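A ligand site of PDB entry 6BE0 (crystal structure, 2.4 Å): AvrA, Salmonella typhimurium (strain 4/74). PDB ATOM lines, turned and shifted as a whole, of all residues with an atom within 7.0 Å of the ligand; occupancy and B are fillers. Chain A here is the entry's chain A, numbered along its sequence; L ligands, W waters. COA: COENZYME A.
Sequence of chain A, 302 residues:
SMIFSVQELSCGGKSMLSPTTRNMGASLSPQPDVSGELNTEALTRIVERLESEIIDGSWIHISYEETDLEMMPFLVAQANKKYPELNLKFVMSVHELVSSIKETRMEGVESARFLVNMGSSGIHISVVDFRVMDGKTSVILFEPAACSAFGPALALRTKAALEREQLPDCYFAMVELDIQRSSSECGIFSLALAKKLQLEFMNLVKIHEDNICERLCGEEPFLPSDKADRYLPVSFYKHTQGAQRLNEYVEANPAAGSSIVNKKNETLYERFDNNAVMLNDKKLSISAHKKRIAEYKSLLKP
The backbone NH (N) of Gln 244 sits at hydrogen-bond distance from an oxygen (O9A) of the ligand (2.8 Å).
An oxygen (O4B) of the ligand sits at hydrogen-bond distance from the guanidinium group (NH1) of Arg 181.
An oxygen (O9A) of the ligand lies within hydrogen-bond range of the backbone NH (N) of Ala 243, 2.9 Å away.
The backbone carbonyl oxygen (O) of Ala 243 lies close to the side-chain amide oxygen (OD1) of Asn 247 (3.2 Å).
N of Ser 182 sits at hydrogen-bond distance from OE1 of Gln 241 (2.9 Å).
The side-chain hydroxyl (OG) of Ser 182 sits at hydrogen-bond distance from the side-chain carboxylate (OE2) of Glu 185 (2.8 Å).
The backbone NH (N) of Arg 181 is in hydrogen-bond range of the side-chain amide oxygen (OE1) of Gln 241 (2.6 Å).
NE2 of Gln 180 is in hydrogen-bond range of O of Ser 182, 3.1 Å away.
Ser 182 touches the ligand.
O of Gln 241 touches C1B of the ligand, at 3.6 Å.
Gly 242 touches the ligand (C to O9A, 3.3 Å).
CD2 of Leu 284 touches N3A of the ligand, at 3.6 Å.
O of Ser 285 touches C2A of the ligand (3.99 Å).
Along chain A the residues within 4 Å of the ligand span positions 181 to 285.
The nearest printed residue that does not touch the ligand is Lys 283 (4.1 Å).
Water W1 lies within hydrogen-bond range of N of Ser 285 and N3A of the ligand.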
ATOM      1  N   TRP A  59       5.938  15.045 -28.040  1.00  0.00           N
ATOM      2  CA  TRP A  59       5.876  16.462 -27.685  1.00  0.00           C
ATOM      3  C   TRP A  59       5.673  16.675 -26.194  1.00  0.00           C
ATOM      4  O   TRP A  59       6.138  17.664 -25.629  1.00  0.00           O
ATOM      5  CB  TRP A  59       4.731  17.153 -28.448  1.00  0.00           C
ATOM      6  CG  TRP A  59       3.367  16.580 -28.144  1.00  0.00           C
ATOM      7  CD1 TRP A  59       2.760  15.539 -28.774  1.00  0.00           C
ATOM      8  CD2 TRP A  59       2.456  17.020 -27.131  1.00  0.00           C
ATOM      9  NE1 TRP A  59       1.523  15.297 -28.229  1.00  0.00           N
ATOM     10  CE2 TRP A  59       1.318  16.197 -27.213  1.00  0.00           C
ATOM     11  CE3 TRP A  59       2.496  18.031 -26.166  1.00  0.00           C
ATOM     12  CZ2 TRP A  59       0.222  16.363 -26.367  1.00  0.00           C
ATOM     13  CZ3 TRP A  59       1.402  18.184 -25.326  1.00  0.00           C
ATOM     14  CH2 TRP A  59       0.279  17.352 -25.432  1.00  0.00           C
ATOM     15  N   ILE A  60       4.966  15.750 -25.553  1.00  0.00           N
ATOM     16  CA  ILE A  60       4.537  15.938 -24.182  1.00  0.00           C
ATOM     17  C   ILE A  60       5.699  15.938 -23.178  1.00  0.00           C
ATOM     18  O   ILE A  60       5.611  16.609 -22.152  1.00  0.00           O
ATOM     19  CB  ILE A  60       3.511  14.854 -23.772  1.00  0.00           C
ATOM     20  CG1 ILE A  60       2.952  15.169 -22.387  1.00  0.00           C
ATOM     21  CG2 ILE A  60       4.129  13.468 -23.816  1.00  0.00           C
ATOM     22  CD1 ILE A  60       1.531  14.682 -22.170  1.00  0.00           C
ATOM     23  N   GLN A 180      -2.785  27.127 -18.648  1.00  0.00           N
ATOM     24  CA  GLN A 180      -1.640  26.336 -19.080  1.00  0.00           C
ATOM     25  C   GLN A 180      -1.450  25.163 -18.125  1.00  0.00           C
ATOM     26  O   GLN A 180      -1.427  25.345 -16.911  1.00  0.00           O
ATOM     27  CB  GLN A 180      -0.357  27.168 -19.126  1.00  0.00           C
ATOM     28  CG  GLN A 180       0.881  26.356 -19.508  1.00  0.00           C
ATOM     29  CD  GLN A 180       2.172  27.111 -19.289  1.00  0.00           C
ATOM     30  OE1 GLN A 180       2.199  28.336 -19.315  1.00  0.00           O
ATOM     31  NE2 GLN A 180       3.257  26.368 -19.060  1.00  0.00           N
ATOM     32  N   ARG A 181      -1.317  23.976 -18.699  1.00  0.00           N
ATOM     33  CA  ARG A 181      -1.075  22.761 -17.918  1.00  0.00           C
ATOM     34  C   ARG A 181       0.149  22.026 -18.468  1.00  0.00           C
ATOM     35  O   ARG A 181       0.785  21.252 -17.754  1.00  0.00           O
ATOM     36  CB  ARG A 181      -2.296  21.852 -17.937  1.00  0.00           C
ATOM     37  CG  ARG A 181      -3.605  22.549 -17.574  1.00  0.00           C
ATOM     38  CD  ARG A 181      -3.645  22.961 -16.117  1.00  0.00           C
ATOM     39  NE  ARG A 181      -4.847  23.729 -15.795  1.00  0.00           N
ATOM     40  CZ  ARG A 181      -6.069  23.217 -15.729  1.00  0.00           C
ATOM     41  NH1 ARG A 181      -6.287  21.929 -15.982  1.00  0.00           N
ATOM     42  NH2 ARG A 181      -7.095  23.993 -15.402  1.00  0.00           N
ATOM     43  N   SER A 182       0.458  22.256 -19.747  1.00  0.00           N
ATOM     44  CA  SER A 182       1.646  21.677 -20.356  1.00  0.00           C
ATOM     45  C   SER A 182       2.893  22.276 -19.693  1.00  0.00           C
ATOM     46  O   SER A 182       2.811  23.313 -19.032  1.00  0.00           O
ATOM     47  CB  SER A 182       1.663  21.905 -21.864  1.00  0.00           C
ATOM     48  OG  SER A 182       1.616  23.278 -22.182  1.00  0.00           O
ATOM     49  N   SER A 183       4.028  21.625 -19.888  1.00  0.00           N
ATOM     50  CA  SER A 183       5.202  21.878 -19.059  1.00  0.00           C
ATOM     51  C   SER A 183       6.088  23.041 -19.511  1.00  0.00           C
ATOM     52  O   SER A 183       6.818  23.613 -18.697  1.00  0.00           O
ATOM     53  CB  SER A 183       6.056  20.607 -19.000  1.00  0.00           C
ATOM     54  OG  SER A 183       6.468  20.207 -20.299  1.00  0.00           O
ATOM     55  N   GLU A 185       5.180  25.723 -22.141  1.00  0.00           N
ATOM     56  CA  GLU A 185       4.487  26.604 -23.071  1.00  0.00           C
ATOM     57  C   GLU A 185       4.248  28.012 -22.518  1.00  0.00           C
ATOM     58  O   GLU A 185       3.397  28.745 -23.015  1.00  0.00           O
ATOM     59  CB  GLU A 185       3.149  25.982 -23.487  1.00  0.00           C
ATOM     60  CG  GLU A 185       3.266  24.915 -24.573  1.00  0.00           C
ATOM     61  CD  GLU A 185       4.352  23.897 -24.268  1.00  0.00           C
ATOM     62  OE1 GLU A 185       5.402  23.929 -24.930  1.00  0.00           O
ATOM     63  OE2 GLU A 185       4.143  23.062 -23.364  1.00  0.00           O
ATOM     64  N   GLN A 241      -5.975  24.499 -21.696  1.00  0.00           N
ATOM     65  CA  GLN A 241      -5.592  23.098 -21.721  1.00  0.00           C
ATOM     66  C   GLN A 241      -6.340  22.315 -20.642  1.00  0.00           C
ATOM     67  O   GLN A 241      -5.753  21.891 -19.647  1.00  0.00           O
ATOM     68  CB  GLN A 241      -4.081  22.961 -21.539  1.00  0.00           C
ATOM     69  CG  GLN A 241      -3.289  23.493 -22.724  1.00  0.00           C
ATOM     70  CD  GLN A 241      -1.806  23.614 -22.446  1.00  0.00           C
ATOM     71  OE1 GLN A 241      -1.382  23.851 -21.321  1.00  0.00           O
ATOM     72  NE2 GLN A 241      -0.999  23.430 -23.489  1.00  0.00           N
ATOM     73  N   GLY A 242      -7.637  22.128 -20.855  1.00  0.00           N
ATOM     74  CA  GLY A 242      -8.472  21.424 -19.896  1.00  0.00           C
ATOM     75  C   GLY A 242      -9.947  21.682 -20.131  1.00  0.00           C
ATOM     76  O   GLY A 242     -10.406  22.828 -20.037  1.00  0.00           O
ATOM     77  N   ALA A 243     -10.692  20.634 -20.434  1.00  0.00           N
ATOM     78  CA  ALA A 243     -12.128  20.739 -20.683  1.00  0.00           C
ATOM     79  C   ALA A 243     -12.853  21.216 -19.422  1.00  0.00           C
ATOM     80  O   ALA A 243     -13.783  22.032 -19.508  1.00  0.00           O
ATOM     81  CB  ALA A 243     -12.684  19.408 -21.151  1.00  0.00           C
ATOM     82  N   GLN A 244     -12.437  20.711 -18.275  1.00  0.00           N
ATOM     83  CA  GLN A 244     -13.026  21.110 -16.997  1.00  0.00           C
ATOM     84  C   GLN A 244     -12.800  22.598 -16.759  1.00  0.00           C
ATOM     85  O   GLN A 244     -13.696  23.296 -16.282  1.00  0.00           O
ATOM     86  CB  GLN A 244     -12.425  20.293 -15.855  1.00  0.00           C
ATOM     87  CG  GLN A 244     -12.987  20.653 -14.482  1.00  0.00           C
ATOM     88  CD  GLN A 244     -14.479  20.398 -14.364  1.00  0.00           C
ATOM     89  OE1 GLN A 244     -14.999  19.407 -14.896  1.00  0.00           O
ATOM     90  NE2 GLN A 244     -15.182  21.298 -13.683  1.00  0.00           N
ATOM     91  N   ARG A 245     -11.611  23.067 -17.099  1.00  0.00           N
ATOM     92  CA  ARG A 245     -11.262  24.474 -16.909  1.00  0.00           C
ATOM     93  C   ARG A 245     -12.155  25.385 -17.748  1.00  0.00           C
ATOM     94  O   ARG A 245     -12.534  26.476 -17.320  1.00  0.00           O
ATOM     95  CB  ARG A 245      -9.793  24.710 -17.246  1.00  0.00           C
ATOM     96  CG  ARG A 245      -9.315  26.141 -17.055  1.00  0.00           C
ATOM     97  CD  ARG A 245      -9.373  26.590 -15.598  1.00  0.00           C
ATOM     98  NE  ARG A 245      -9.074  28.018 -15.473  1.00  0.00           N
ATOM     99  CZ  ARG A 245      -9.979  28.992 -15.581  1.00  0.00           C
ATOM    100  NH1 ARG A 245     -11.253  28.701 -15.818  1.00  0.00           N
ATOM    101  NH2 ARG A 245      -9.611  30.257 -15.452  1.00  0.00           N
ATOM    102  N   LEU A 246     -12.468  24.934 -18.965  1.00  0.00           N
ATOM    103  CA  LEU A 246     -13.365  25.685 -19.835  1.00  0.00           C
ATOM    104  C   LEU A 246     -14.783  25.673 -19.279  1.00  0.00           C
ATOM    105  O   LEU A 246     -15.492  26.684 -19.369  1.00  0.00           O
ATOM    106  CB  LEU A 246     -13.349  25.108 -21.255  1.00  0.00           C
ATOM    107  CG  LEU A 246     -12.128  25.414 -22.126  1.00  0.00           C
ATOM    108  CD1 LEU A 246     -12.235  24.683 -23.455  1.00  0.00           C
ATOM    109  CD2 LEU A 246     -11.984  26.914 -22.364  1.00  0.00           C
ATOM    110  N   ASN A 247     -15.202  24.542 -18.725  1.00  0.00           N
ATOM    111  CA  ASN A 247     -16.520  24.438 -18.120  1.00  0.00           C
ATOM    112  C   ASN A 247     -16.660  25.404 -16.947  1.00  0.00           C
ATOM    113  O   ASN A 247     -17.758  25.876 -16.646  1.00  0.00           O
ATOM    114  CB  ASN A 247     -16.783  23.010 -17.627  1.00  0.00           C
ATOM    115  CG  ASN A 247     -16.798  22.002 -18.757  1.00  0.00           C
ATOM    116  OD1 ASN A 247     -16.938  22.350 -19.929  1.00  0.00           O
ATOM    117  ND2 ASN A 247     -16.661  20.724 -18.404  1.00  0.00           N
ATOM    118  N   PHE A 272     -11.772  24.007 -29.166  1.00  0.00           N
ATOM    119  CA  PHE A 272     -11.037  23.188 -28.201  1.00  0.00           C
ATOM    120  C   PHE A 272     -10.903  21.751 -28.701  1.00  0.00           C
ATOM    121  O   PHE A 272      -9.845  21.146 -28.572  1.00  0.00           O
ATOM    122  CB  PHE A 272     -11.743  23.200 -26.840  1.00  0.00           C
ATOM    123  CG  PHE A 272     -11.171  22.216 -25.859  1.00  0.00           C
ATOM    124  CD1 PHE A 272     -10.015  22.507 -25.152  1.00  0.00           C
ATOM    125  CD2 PHE A 272     -11.793  20.998 -25.639  1.00  0.00           C
ATOM    126  CE1 PHE A 272      -9.478  21.600 -24.248  1.00  0.00           C
ATOM    127  CE2 PHE A 272     -11.267  20.083 -24.738  1.00  0.00           C
ATOM    128  CZ  PHE A 272     -10.113  20.394 -24.042  1.00  0.00           C
ATOM    129  N   LYS A 282      -6.678   9.656 -22.900  1.00  0.00           N
ATOM    130  CA  LYS A 282      -6.878  10.953 -22.266  1.00  0.00           C
ATOM    131  C   LYS A 282      -6.806  12.068 -23.295  1.00  0.00           C
ATOM    132  O   LYS A 282      -5.810  12.195 -24.013  1.00  0.00           O
ATOM    133  CB  LYS A 282      -5.850  11.179 -21.158  1.00  0.00           C
ATOM    134  CG  LYS A 282      -5.999  10.249 -19.963  1.00  0.00           C
ATOM    135  CD  LYS A 282      -4.985  10.560 -18.872  1.00  0.00           C
ATOM    136  CE  LYS A 282      -5.155   9.655 -17.671  1.00  0.00           C
ATOM    137  NZ  LYS A 282      -4.142   9.932 -16.609  1.00  0.00           N
ATOM    138  N   LYS A 283      -7.866  12.872 -23.375  1.00  0.00           N
ATOM    139  CA  LYS A 283      -7.934  13.945 -24.356  1.00  0.00           C
ATOM    140  C   LYS A 283      -7.114  15.147 -23.913  1.00  0.00           C
ATOM    141  O   LYS A 283      -7.426  15.797 -22.915  1.00  0.00           O
ATOM    142  CB  LYS A 283      -9.390  14.362 -24.600  1.00  0.00           C
ATOM    143  CG  LYS A 283      -9.556  15.328 -25.762  1.00  0.00           C
ATOM    144  CD  LYS A 283     -11.025  15.503 -26.156  1.00  0.00           C
ATOM    145  CE  LYS A 283     -11.782  16.363 -25.161  1.00  0.00           C
ATOM    146  NZ  LYS A 283     -13.163  16.666 -25.620  1.00  0.00           N
ATOM    147  N   LEU A 284      -6.044  15.428 -24.657  1.00  0.00           N
ATOM    148  CA  LEU A 284      -5.163  16.561 -24.376  1.00  0.00           C
ATOM    149  C   LEU A 284      -5.252  17.594 -25.483  1.00  0.00           C
ATOM    150  O   LEU A 284      -5.578  17.270 -26.621  1.00  0.00           O
ATOM    151  CB  LEU A 284      -3.719  16.086 -24.217  1.00  0.00           C
ATOM    152  CG  LEU A 284      -3.442  15.103 -23.073  1.00  0.00           C
ATOM    153  CD1 LEU A 284      -1.991  14.654 -23.131  1.00  0.00           C
ATOM    154  CD2 LEU A 284      -3.768  15.722 -21.732  1.00  0.00           C
ATOM    155  N   SER A 285      -4.935  18.838 -25.146  1.00  0.00           N
ATOM    156  CA  SER A 285      -4.920  19.931 -26.119  1.00  0.00           C
ATOM    157  C   SER A 285      -3.506  20.230 -26.578  1.00  0.00           C
ATOM    158  O   SER A 285      -2.603  20.446 -25.765  1.00  0.00           O
ATOM    159  CB  SER A 285      -5.563  21.190 -25.534  1.00  0.00           C
ATOM    160  OG  SER A 285      -5.416  22.288 -26.414  1.00  0.00           O
ATOM    161  N   ILE A 286      -3.312  20.246 -27.904  1.00  0.00           N
ATOM    162  CA  ILE A 286      -2.047  20.653 -28.500  1.00  0.00           C
ATOM    163  C   ILE A 286      -2.196  22.017 -29.156  1.00  0.00           C
ATOM    164  O   ILE A 286      -1.475  22.337 -30.107  1.00  0.00           O
ATOM    165  CB  ILE A 286      -1.549  19.620 -29.536  1.00  0.00           C
ATOM    166  CG1 ILE A 286      -2.559  19.469 -30.679  1.00  0.00           C
ATOM    167  CG2 ILE A 286      -1.289  18.285 -28.863  1.00  0.00           C
ATOM    168  CD1 ILE A 286      -2.012  18.731 -31.879  1.00  0.00           C
ATOM    169  N   HIS A 289       0.847  24.218 -28.646  1.00  0.00           N
ATOM    170  CA  HIS A 289       1.947  23.643 -29.416  1.00  0.00           C
ATOM    171  C   HIS A 289       1.789  23.946 -30.902  1.00  0.00           C
ATOM    172  O   HIS A 289       2.778  24.185 -31.606  1.00  0.00           O
ATOM    173  CB  HIS A 289       2.031  22.130 -29.191  1.00  0.00           C
ATOM    174  CG  HIS A 289       2.569  21.753 -27.847  1.00  0.00           C
ATOM    175  ND1 HIS A 289       1.811  21.815 -26.697  1.00  0.00           N
ATOM    176  CD2 HIS A 289       3.788  21.320 -27.464  1.00  0.00           C
ATOM    177  CE1 HIS A 289       2.541  21.421 -25.673  1.00  0.00           C
ATOM    178  NE2 HIS A 289       3.753  21.121 -26.107  1.00  0.00           N
HETATM  179  N1A COA L   1      -1.200  19.003 -21.848  1.00  0.00           N
HETATM  180  C2A COA L   1      -2.545  19.263 -21.952  1.00  0.00           C
HETATM  181  N3A COA L   1      -3.346  19.155 -20.861  1.00  0.00           N
HETATM  182  C4A COA L   1      -2.828  18.788 -19.646  1.00  0.00           C
HETATM  183  C5A COA L   1      -1.504  18.528 -19.535  1.00  0.00           C
HETATM  184  C6A COA L   1      -0.691  18.647 -20.659  1.00  0.00           C
HETATM  185  N6A COA L   1       0.633  18.534 -21.175  1.00  0.00           N
HETATM  186  N7A COA L   1      -1.243  18.186 -18.242  1.00  0.00           N
HETATM  187  C8A COA L   1      -2.418  18.242 -17.547  1.00  0.00           C
HETATM  188  N9A COA L   1      -3.392  18.609 -18.410  1.00  0.00           N
HETATM  189  C1B COA L   1      -4.783  18.791 -18.134  1.00  0.00           C
HETATM  190  C2B COA L   1      -5.492  17.806 -18.638  1.00  0.00           C
HETATM  191  O2B COA L   1      -6.049  18.186 -19.929  1.00  0.00           O
HETATM  192  C3B COA L   1      -6.684  17.543 -17.563  1.00  0.00           C
HETATM  193  O3B COA L   1      -7.697  18.541 -17.682  1.00  0.00           O
HETATM  194  P3B COA L   1      -9.192  18.086 -18.097  1.00  0.00           P
HETATM  195  O7A COA L   1      -9.210  17.675 -19.547  1.00  0.00           O
HETATM  196  O8A COA L   1      -9.631  16.934 -17.239  1.00  0.00           O
HETATM  197  O9A COA L   1     -10.137  19.252 -17.890  1.00  0.00           O
HETATM  198  C4B COA L   1      -6.071  17.645 -16.361  1.00  0.00           C
HETATM  199  O4B COA L   1      -5.022  18.730 -16.566  1.00  0.00           O
HETATM  200  C5B COA L   1      -5.404  16.317 -15.990  1.00  0.00           C
HETATM  201  O5B COA L   1      -4.573  16.497 -14.847  1.00  0.00           O
HETATM  202  P1A COA L   1      -5.006  15.836 -13.447  1.00  0.00           P
HETATM  203  O1A COA L   1      -6.515  15.700 -13.387  1.00  0.00           O
HETATM  204  O2A COA L   1      -4.350  14.474 -13.328  1.00  0.00           O
HETATM  205  O3A COA L   1      -4.515  16.767 -12.266  1.00  0.00           O
HETATM  206  O   HOH W   1      -5.588  19.784 -22.569  1.00  0.00           O
